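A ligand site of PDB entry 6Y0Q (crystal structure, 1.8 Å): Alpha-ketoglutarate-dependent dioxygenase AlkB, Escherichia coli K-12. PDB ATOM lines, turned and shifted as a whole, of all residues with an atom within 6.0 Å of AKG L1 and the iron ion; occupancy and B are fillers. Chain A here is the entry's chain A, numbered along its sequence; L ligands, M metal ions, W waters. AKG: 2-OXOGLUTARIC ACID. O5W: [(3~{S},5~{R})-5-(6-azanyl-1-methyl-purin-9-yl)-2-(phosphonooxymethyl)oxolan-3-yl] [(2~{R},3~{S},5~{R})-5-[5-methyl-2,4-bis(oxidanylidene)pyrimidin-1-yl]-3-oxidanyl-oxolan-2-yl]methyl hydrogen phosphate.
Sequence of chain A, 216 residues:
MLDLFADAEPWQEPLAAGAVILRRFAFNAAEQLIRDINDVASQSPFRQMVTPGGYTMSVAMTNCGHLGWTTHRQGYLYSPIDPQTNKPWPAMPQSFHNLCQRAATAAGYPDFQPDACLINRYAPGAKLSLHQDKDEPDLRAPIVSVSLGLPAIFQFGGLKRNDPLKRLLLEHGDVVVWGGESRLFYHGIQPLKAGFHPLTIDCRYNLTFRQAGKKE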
ATOM      1  N   MET A  61      11.733 -12.288   9.513  1.00  0.00           N
ATOM      2  CA  MET A  61      11.975 -12.523  10.927  1.00  0.00           C
ATOM      3  C   MET A  61      13.462 -12.636  11.215  1.00  0.00           C
ATOM      4  O   MET A  61      14.275 -13.012  10.357  1.00  0.00           O
ATOM      5  CB  MET A  61      11.304 -13.827  11.412  1.00  0.00           C
ATOM      6  CG  MET A  61       9.793 -13.780  11.456  1.00  0.00           C
ATOM      7  SD  MET A  61       9.098 -15.413  11.693  1.00  0.00           S
ATOM      8  CE  MET A  61       7.432 -14.994  12.210  1.00  0.00           C
ATOM      9  N   LEU A 118      11.614 -12.812  19.364  1.00  0.00           N
ATOM     10  CA  LEU A 118      11.367 -12.901  17.939  1.00  0.00           C
ATOM     11  C   LEU A 118      11.049 -11.512  17.409  1.00  0.00           C
ATOM     12  O   LEU A 118      10.220 -10.802  17.987  1.00  0.00           O
ATOM     13  CB  LEU A 118      10.215 -13.867  17.674  1.00  0.00           C
ATOM     14  CG  LEU A 118       9.807 -14.083  16.224  1.00  0.00           C
ATOM     15  CD1 LEU A 118      10.944 -14.704  15.422  1.00  0.00           C
ATOM     16  CD2 LEU A 118       8.563 -14.962  16.185  1.00  0.00           C
ATOM     17  N   ASN A 120       9.709  -9.493  14.107  1.00  0.00           N
ATOM     18  CA  ASN A 120       8.990  -9.584  12.849  1.00  0.00           C
ATOM     19  C   ASN A 120       9.014  -8.242  12.122  1.00  0.00           C
ATOM     20  O   ASN A 120       8.789  -7.199  12.740  1.00  0.00           O
ATOM     21  CB  ASN A 120       7.520  -9.970  13.060  1.00  0.00           C
ATOM     22  CG  ASN A 120       7.341 -11.345  13.659  1.00  0.00           C
ATOM     23  OD1 ASN A 120       8.299 -12.023  14.022  1.00  0.00           O
ATOM     24  ND2 ASN A 120       6.092 -11.773  13.768  1.00  0.00           N
ATOM     25  N   TYR A 122       7.139  -6.384   8.834  1.00  0.00           N
ATOM     26  CA  TYR A 122       6.027  -6.431   7.898  1.00  0.00           C
ATOM     27  C   TYR A 122       6.173  -5.295   6.895  1.00  0.00           C
ATOM     28  O   TYR A 122       6.105  -4.123   7.275  1.00  0.00           O
ATOM     29  CB  TYR A 122       4.678  -6.299   8.612  1.00  0.00           C
ATOM     30  CG  TYR A 122       4.369  -7.378   9.623  1.00  0.00           C
ATOM     31  CD1 TYR A 122       4.897  -7.331  10.906  1.00  0.00           C
ATOM     32  CD2 TYR A 122       3.520  -8.415   9.305  1.00  0.00           C
ATOM     33  CE1 TYR A 122       4.602  -8.311  11.834  1.00  0.00           C
ATOM     34  CE2 TYR A 122       3.224  -9.401  10.221  1.00  0.00           C
ATOM     35  CZ  TYR A 122       3.767  -9.342  11.490  1.00  0.00           C
ATOM     36  OH  TYR A 122       3.448 -10.337  12.387  1.00  0.00           O
ATOM     37  N   LEU A 128       0.185 -12.477   8.512  1.00  0.00           N
ATOM     38  CA  LEU A 128       0.528 -13.673   9.282  1.00  0.00           C
ATOM     39  C   LEU A 128      -0.781 -14.389   9.590  1.00  0.00           C
ATOM     40  O   LEU A 128      -1.620 -13.857  10.317  1.00  0.00           O
ATOM     41  CB  LEU A 128       1.279 -13.304  10.556  1.00  0.00           C
ATOM     42  CG  LEU A 128       1.758 -14.445  11.430  1.00  0.00           C
ATOM     43  CD1 LEU A 128       2.688 -15.366  10.649  1.00  0.00           C
ATOM     44  CD2 LEU A 128       2.462 -13.883  12.658  1.00  0.00           C
ATOM     45  N   HIS A 131      -2.641 -18.738  13.950  1.00  0.00           N
ATOM     46  CA  HIS A 131      -1.826 -19.780  14.548  1.00  0.00           C
ATOM     47  C   HIS A 131      -1.872 -19.622  16.057  1.00  0.00           C
ATOM     48  O   HIS A 131      -2.272 -18.585  16.589  1.00  0.00           O
ATOM     49  CB  HIS A 131      -0.369 -19.679  14.091  1.00  0.00           C
ATOM     50  CG  HIS A 131       0.289 -18.426  14.558  1.00  0.00           C
ATOM     51  ND1 HIS A 131       0.152 -17.229  13.899  1.00  0.00           N
ATOM     52  CD2 HIS A 131       1.037 -18.167  15.664  1.00  0.00           C
ATOM     53  CE1 HIS A 131       0.819 -16.287  14.557  1.00  0.00           C
ATOM     54  NE2 HIS A 131       1.356 -16.836  15.639  1.00  0.00           N
ATOM     55  N   GLN A 132      -1.429 -20.675  16.746  1.00  0.00           N
ATOM     56  CA  GLN A 132      -1.120 -20.646  18.157  1.00  0.00           C
ATOM     57  C   GLN A 132       0.395 -20.701  18.364  1.00  0.00           C
ATOM     58  O   GLN A 132       1.125 -21.270  17.548  1.00  0.00           O
ATOM     59  CB  GLN A 132      -1.751 -21.823  18.910  1.00  0.00           C
ATOM     60  CG  GLN A 132      -3.256 -21.845  18.938  1.00  0.00           C
ATOM     61  CD  GLN A 132      -3.782 -23.102  19.600  1.00  0.00           C
ATOM     62  OE1 GLN A 132      -3.486 -24.221  19.176  1.00  0.00           O
ATOM     63  NE2 GLN A 132      -4.570 -22.933  20.657  1.00  0.00           N
ATOM     64  N   ASP A 133       0.833 -20.136  19.481  1.00  0.00           N
ATOM     65  CA  ASP A 133       2.229 -20.183  19.926  1.00  0.00           C
ATOM     66  C   ASP A 133       2.317 -21.265  21.000  1.00  0.00           C
ATOM     67  O   ASP A 133       1.971 -21.031  22.157  1.00  0.00           O
ATOM     68  CB  ASP A 133       2.653 -18.830  20.478  1.00  0.00           C
ATOM     69  CG  ASP A 133       2.989 -17.814  19.378  1.00  0.00           C
ATOM     70  OD1 ASP A 133       2.135 -17.576  18.495  1.00  0.00           O
ATOM     71  OD2 ASP A 133       4.107 -17.274  19.407  1.00  0.00           O
ATOM     72  N   SER A 145       4.292  -8.580  23.681  1.00  0.00           N
ATOM     73  CA  SER A 145       4.327  -8.140  22.293  1.00  0.00           C
ATOM     74  C   SER A 145       4.439  -6.615  22.218  1.00  0.00           C
ATOM     75  O   SER A 145       3.677  -5.902  22.871  1.00  0.00           O
ATOM     76  CB  SER A 145       3.063  -8.585  21.560  1.00  0.00           C
ATOM     77  OG  SER A 145       2.914  -7.892  20.328  1.00  0.00           O
ATOM     78  N   SER A 147       4.703  -3.337  19.452  1.00  0.00           N
ATOM     79  CA  SER A 147       4.443  -2.921  18.075  1.00  0.00           C
ATOM     80  C   SER A 147       5.135  -1.586  17.785  1.00  0.00           C
ATOM     81  O   SER A 147       5.084  -0.667  18.600  1.00  0.00           O
ATOM     82  CB  SER A 147       2.939  -2.800  17.815  1.00  0.00           C
ATOM     83  OG  SER A 147       2.294  -4.071  17.821  1.00  0.00           O
ATOM     84  N   PHE A 154      -4.723  -6.707  14.266  1.00  0.00           N
ATOM     85  CA  PHE A 154      -4.461  -7.976  14.923  1.00  0.00           C
ATOM     86  C   PHE A 154      -5.790  -8.705  15.075  1.00  0.00           C
ATOM     87  O   PHE A 154      -6.766  -8.117  15.548  1.00  0.00           O
ATOM     88  CB  PHE A 154      -3.805  -7.714  16.285  1.00  0.00           C
ATOM     89  CG  PHE A 154      -3.464  -8.948  17.072  1.00  0.00           C
ATOM     90  CD1 PHE A 154      -2.259  -9.582  16.892  1.00  0.00           C
ATOM     91  CD2 PHE A 154      -4.343  -9.455  18.020  1.00  0.00           C
ATOM     92  CE1 PHE A 154      -1.935 -10.705  17.622  1.00  0.00           C
ATOM     93  CE2 PHE A 154      -4.025 -10.578  18.743  1.00  0.00           C
ATOM     94  CZ  PHE A 154      -2.829 -11.198  18.558  1.00  0.00           C
ATOM     95  N   LEU A 170      -3.458  -2.351  16.383  1.00  0.00           N
ATOM     96  CA  LEU A 170      -2.242  -2.165  17.155  1.00  0.00           C
ATOM     97  C   LEU A 170      -1.416  -1.059  16.499  1.00  0.00           C
ATOM     98  O   LEU A 170      -1.108  -1.136  15.304  1.00  0.00           O
ATOM     99  CB  LEU A 170      -1.444  -3.460  17.255  1.00  0.00           C
ATOM    100  CG  LEU A 170      -2.078  -4.576  18.089  1.00  0.00           C
ATOM    101  CD1 LEU A 170      -1.198  -5.807  18.073  1.00  0.00           C
ATOM    102  CD2 LEU A 170      -2.311  -4.108  19.511  1.00  0.00           C
ATOM    103  N   HIS A 187      -4.310 -16.532  16.615  1.00  0.00           N
ATOM    104  CA  HIS A 187      -4.110 -15.113  16.345  1.00  0.00           C
ATOM    105  C   HIS A 187      -3.307 -14.926  15.060  1.00  0.00           C
ATOM    106  O   HIS A 187      -2.609 -15.824  14.592  1.00  0.00           O
ATOM    107  CB  HIS A 187      -3.409 -14.437  17.531  1.00  0.00           C
ATOM    108  CG  HIS A 187      -2.063 -15.017  17.827  1.00  0.00           C
ATOM    109  ND1 HIS A 187      -1.897 -16.157  18.591  1.00  0.00           N
ATOM    110  CD2 HIS A 187      -0.829 -14.638  17.437  1.00  0.00           C
ATOM    111  CE1 HIS A 187      -0.606 -16.439  18.671  1.00  0.00           C
ATOM    112  NE2 HIS A 187       0.060 -15.531  17.991  1.00  0.00           N
ATOM    113  N   GLY A 188      -3.434 -13.724  14.500  1.00  0.00           N
ATOM    114  CA  GLY A 188      -2.732 -13.403  13.274  1.00  0.00           C
ATOM    115  C   GLY A 188      -2.812 -11.921  12.983  1.00  0.00           C
ATOM    116  O   GLY A 188      -3.367 -11.137  13.770  1.00  0.00           O
ATOM    117  N   ILE A 189      -2.255 -11.542  11.843  1.00  0.00           N
ATOM    118  CA  ILE A 189      -2.163 -10.155  11.389  1.00  0.00           C
ATOM    119  C   ILE A 189      -2.710 -10.089   9.971  1.00  0.00           C
ATOM    120  O   ILE A 189      -2.361 -10.915   9.115  1.00  0.00           O
ATOM    121  CB  ILE A 189      -0.706  -9.651  11.426  1.00  0.00           C
ATOM    122  CG1 ILE A 189      -0.209  -9.563  12.869  1.00  0.00           C
ATOM    123  CG2 ILE A 189      -0.552  -8.308  10.704  1.00  0.00           C
ATOM    124  CD1 ILE A 189      -0.744  -8.390  13.638  1.00  0.00           C
ATOM    125  N   ARG A 204       6.244  -2.145   9.544  1.00  0.00           N
ATOM    126  CA  ARG A 204       5.920  -2.398  10.940  1.00  0.00           C
ATOM    127  C   ARG A 204       6.898  -3.414  11.499  1.00  0.00           C
ATOM    128  O   ARG A 204       7.225  -4.396  10.829  1.00  0.00           O
ATOM    129  CB  ARG A 204       4.486  -2.944  11.098  1.00  0.00           C
ATOM    130  CG  ARG A 204       4.138  -3.370  12.509  1.00  0.00           C
ATOM    131  CD  ARG A 204       2.699  -3.900  12.591  1.00  0.00           C
ATOM    132  NE  ARG A 204       2.337  -4.322  13.946  1.00  0.00           N
ATOM    133  CZ  ARG A 204       2.290  -5.588  14.369  1.00  0.00           C
ATOM    134  NH1 ARG A 204       2.572  -6.604  13.553  1.00  0.00           N
ATOM    135  NH2 ARG A 204       1.947  -5.849  15.623  1.00  0.00           N
ATOM    136  N   ASN A 206       7.363  -5.950  14.942  1.00  0.00           N
ATOM    137  CA  ASN A 206       6.780  -6.501  16.151  1.00  0.00           C
ATOM    138  C   ASN A 206       7.833  -7.327  16.864  1.00  0.00           C
ATOM    139  O   ASN A 206       8.526  -8.128  16.236  1.00  0.00           O
ATOM    140  CB  ASN A 206       5.550  -7.353  15.844  1.00  0.00           C
ATOM    141  CG  ASN A 206       4.960  -8.010  17.077  1.00  0.00           C
ATOM    142  OD1 ASN A 206       5.150  -9.198  17.313  1.00  0.00           O
ATOM    143  ND2 ASN A 206       4.235  -7.228  17.868  1.00  0.00           N
ATOM    144  N   THR A 208       8.247 -10.063  20.025  1.00  0.00           N
ATOM    145  CA  THR A 208       7.562 -10.928  20.988  1.00  0.00           C
ATOM    146  C   THR A 208       8.599 -11.611  21.871  1.00  0.00           C
ATOM    147  O   THR A 208       9.408 -12.415  21.381  1.00  0.00           O
ATOM    148  CB  THR A 208       6.646 -11.963  20.315  1.00  0.00           C
ATOM    149  OG1 THR A 208       7.315 -12.612  19.234  1.00  0.00           O
ATOM    150  CG2 THR A 208       5.370 -11.304  19.819  1.00  0.00           C
ATOM    151  N   ARG A 210       9.705 -14.168  24.797  1.00  0.00           N
ATOM    152  CA  ARG A 210       9.270 -15.498  25.180  1.00  0.00           C
ATOM    153  C   ARG A 210      10.204 -16.109  26.219  1.00  0.00           C
ATOM    154  O   ARG A 210      11.406 -15.828  26.237  1.00  0.00           O
ATOM    155  CB  ARG A 210       9.198 -16.404  23.951  1.00  0.00           C
ATOM    156  CG  ARG A 210       8.291 -15.840  22.862  1.00  0.00           C
ATOM    157  CD  ARG A 210       8.956 -15.783  21.491  1.00  0.00           C
ATOM    158  NE  ARG A 210       8.018 -15.215  20.511  1.00  0.00           N
ATOM    159  CZ  ARG A 210       6.962 -15.871  20.028  1.00  0.00           C
ATOM    160  NH1 ARG A 210       6.706 -17.118  20.409  1.00  0.00           N
ATOM    161  NH2 ARG A 210       6.143 -15.268  19.169  1.00  0.00           N
HETATM  162  C1  AKG L   1       4.071 -14.298  16.062  1.00  0.00           C
HETATM  163  O1  AKG L   1       5.125 -14.043  15.423  1.00  0.00           O
HETATM  164  O2  AKG L   1       3.940 -15.398  16.661  1.00  0.00           O
HETATM  165  C2  AKG L   1       2.947 -13.264  16.101  1.00  0.00           C
HETATM  166  O5  AKG L   1       1.857 -13.596  16.428  1.00  0.00           O
HETATM  167  C3  AKG L   1       3.237 -11.811  15.683  1.00  0.00           C
HETATM  168  C4  AKG L   1       2.043 -10.932  16.071  1.00  0.00           C
HETATM  169  C5  AKG L   1       2.260  -9.464  15.663  1.00  0.00           C
HETATM  170  O3  AKG L   1       2.918  -9.181  14.625  1.00  0.00           O
HETATM  171  O4  AKG L   1       1.745  -8.556  16.370  1.00  0.00           O
HETATM  172  C31 O5W L   2      -0.775 -19.859   1.934  1.00  0.00           C
HETATM  173  C32 O5W L   2      -1.785 -20.836   1.423  1.00  0.00           C
HETATM  174  C01 O5W L   2       6.015 -17.639  16.811  1.00  0.00           C
HETATM  175  C03 O5W L   2       4.715 -19.361  15.700  1.00  0.00           C
HETATM  176  C04 O5W L   2       4.001 -19.819  14.558  1.00  0.00           C
HETATM  177  C05 O5W L   2       3.914 -18.990  13.480  1.00  0.00           C
HETATM  178  C07 O5W L   2       2.848 -20.847  12.997  1.00  0.00           C
HETATM  179  C09 O5W L   2       2.879 -19.055  11.243  1.00  0.00           C
HETATM  180  C10 O5W L   2       3.354 -19.969  10.036  1.00  0.00           C
HETATM  181  C11 O5W L   2       2.262 -19.628   8.973  1.00  0.00           C
HETATM  182  C12 O5W L   2       1.143 -19.457   9.642  1.00  0.00           C
HETATM  183  C14 O5W L   2       0.338 -20.703   9.748  1.00  0.00           C
HETATM  184  C24 O5W L   2       2.835 -18.647   4.650  1.00  0.00           C
HETATM  185  C25 O5W L   2       2.317 -17.976   3.358  1.00  0.00           C
HETATM  186  C26 O5W L   2       0.903 -17.269   3.587  1.00  0.00           C
HETATM  187  C27 O5W L   2       0.373 -17.141   2.165  1.00  0.00           C
HETATM  188  C28 O5W L   2       0.974 -18.122   1.465  1.00  0.00           C
HETATM  189  C33 O5W L   2      -1.993 -21.000  -0.047  1.00  0.00           C
HETATM  190  C35 O5W L   2      -0.199 -19.230  -0.477  1.00  0.00           C
HETATM  191  C38 O5W L   2      -2.620 -21.680   2.411  1.00  0.00           C
HETATM  192  C42 O5W L   2       5.151 -17.356  14.569  1.00  0.00           C
HETATM  193  N02 O5W L   2       5.258 -18.138  15.641  1.00  0.00           N
HETATM  194  N06 O5W L   2       3.205 -19.645  12.541  1.00  0.00           N
HETATM  195  N08 O5W L   2       3.335 -20.976  14.242  1.00  0.00           N
HETATM  196  N30 O5W L   2       0.009 -19.066   0.993  1.00  0.00           N
HETATM  197  N34 O5W L   2      -1.202 -20.206  -0.981  1.00  0.00           N
HETATM  198  N41 O5W L   2       4.494 -17.745  13.480  1.00  0.00           N
HETATM  199  N43 O5W L   2       4.838 -20.202  16.867  1.00  0.00           N
HETATM  200  O13 O5W L   2       1.589 -18.962  11.169  1.00  0.00           O
HETATM  201  O15 O5W L   2       1.132 -21.698  10.349  1.00  0.00           O
HETATM  202  O17 O5W L   2      -0.388 -23.712  10.866  1.00  0.00           O
HETATM  203  O18 O5W L   2       2.076 -24.241  10.325  1.00  0.00           O
HETATM  204  O19 O5W L   2       0.262 -23.460   8.698  1.00  0.00           O
HETATM  205  O20 O5W L   2       2.653 -18.334   8.336  1.00  0.00           O
HETATM  206  O22 O5W L   2       0.996 -16.644   7.192  1.00  0.00           O
HETATM  207  O23 O5W L   2       2.877 -17.658   5.688  1.00  0.00           O
HETATM  208  O29 O5W L   2       2.047 -18.857   2.479  1.00  0.00           O
HETATM  209  O36 O5W L   2       0.444 -18.585  -1.234  1.00  0.00           O
HETATM  210  O37 O5W L   2      -2.787 -21.778  -0.450  1.00  0.00           O
HETATM  211  O39 O5W L   2       1.053 -16.053   4.159  1.00  0.00           O
HETATM  212  O40 O5W L   2       0.747 -18.786   6.661  1.00  0.00           O
HETATM  213  P16 O5W L   2       0.765 -23.290  10.065  1.00  0.00           P
HETATM  214  P21 O5W L   2       1.804 -17.827   6.971  1.00  0.00           P
HETATM  215 FE    FE M   1       2.075 -15.784  17.385  1.00  0.00          FE
HETATM  216  O   HOH W   1       0.947  -9.184  18.871  1.00  0.00           O
HETATM  217  O   HOH W   2       2.687 -14.522  19.272  1.00  0.00           O
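The iron ion is bound by O2 of AKG L1 (2.0 Å). The iron ion is bound by OD1 of Asp 133 (2.1 Å). The iron ion is bound by NE2 of His 187 (2.1 Å). A ring nitrogen (NE2) of His 131 binds the iron ion. Water W2 binds the iron ion, 2.4 Å away. O5 of AKG L1 is bound to the iron ion (2.4 Å).
Of the 19 residues printed, 3 come within 4 Å of the iron ion. The nearest printed residue that does not touch the iron ion is Arg 210 (4.5 Å).
O3 of AKG L1 is in hydrogen-bond range of OH of Tyr 122 (2.6 Å). O3 of AKG L1 is in salt-bridge range of NH1 of Arg 204 (2.8 Å). An oxygen (O1) of AKG L1 lies within hydrogen-bond range of the side-chain amide nitrogen (ND2) of Asn 120, at 3.0 Å. An oxygen (O4) of AKG L1 is in hydrogen-bond range of the side-chain amide nitrogen of Asn 206 (3.2 Å). The guanidinium group (NH2) of Arg 210 sits close to an oxygen (O2) of AKG L1 (3.3 Å).
The side-chain carboxylate of Asp 133 is in salt-bridge range of the guanidinium group of Arg 210 (2.8 Å). The backbone NH (N) of Tyr 122 lies within hydrogen-bond range of the backbone carbonyl oxygen (O) of Arg 204 (2.8 Å). The side-chain hydroxyl (OH) of Tyr 122 lies within hydrogen-bond range of the side-chain amide nitrogen (ND2) of Asn 120 (3.3 Å). The side-chain hydroxyl (OG) of Ser 147 lies within hydrogen-bond range of the guanidinium group (NH2) of Arg 204 (2.8 Å). The backbone NH (N) of Asn 120 sits at hydrogen-bond distance from the backbone carbonyl oxygen (O) of Asn 206 (2.8 Å). ND2 of Asn 206 is in hydrogen-bond range of OG of Ser 145, at 2.9 Å. NH2 of Arg 210 sits at hydrogen-bond distance from OG1 of Thr 208, 2.9 Å away. The backbone carbonyl oxygen (O) of Leu 118 is in hydrogen-bond range of the backbone NH (N) of Thr 208, at 2.9 Å.
Water W1 bridges O4 of AKG L1 (2.7 Å) and OG of Ser 145 (2.8 Å).
Residues that only touch AKG L1: Leu 118 (3.6 Å), Leu 128 (3.5 Å) and Ile 189 (3.6 Å). Hydrophobic or aromatic side chains that line AKG L1: Leu 118, Tyr 122, Leu 128, His 131, His 187 and Ile 189. Of the 19 residues printed, 11 come within 4 Å of AKG L1.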
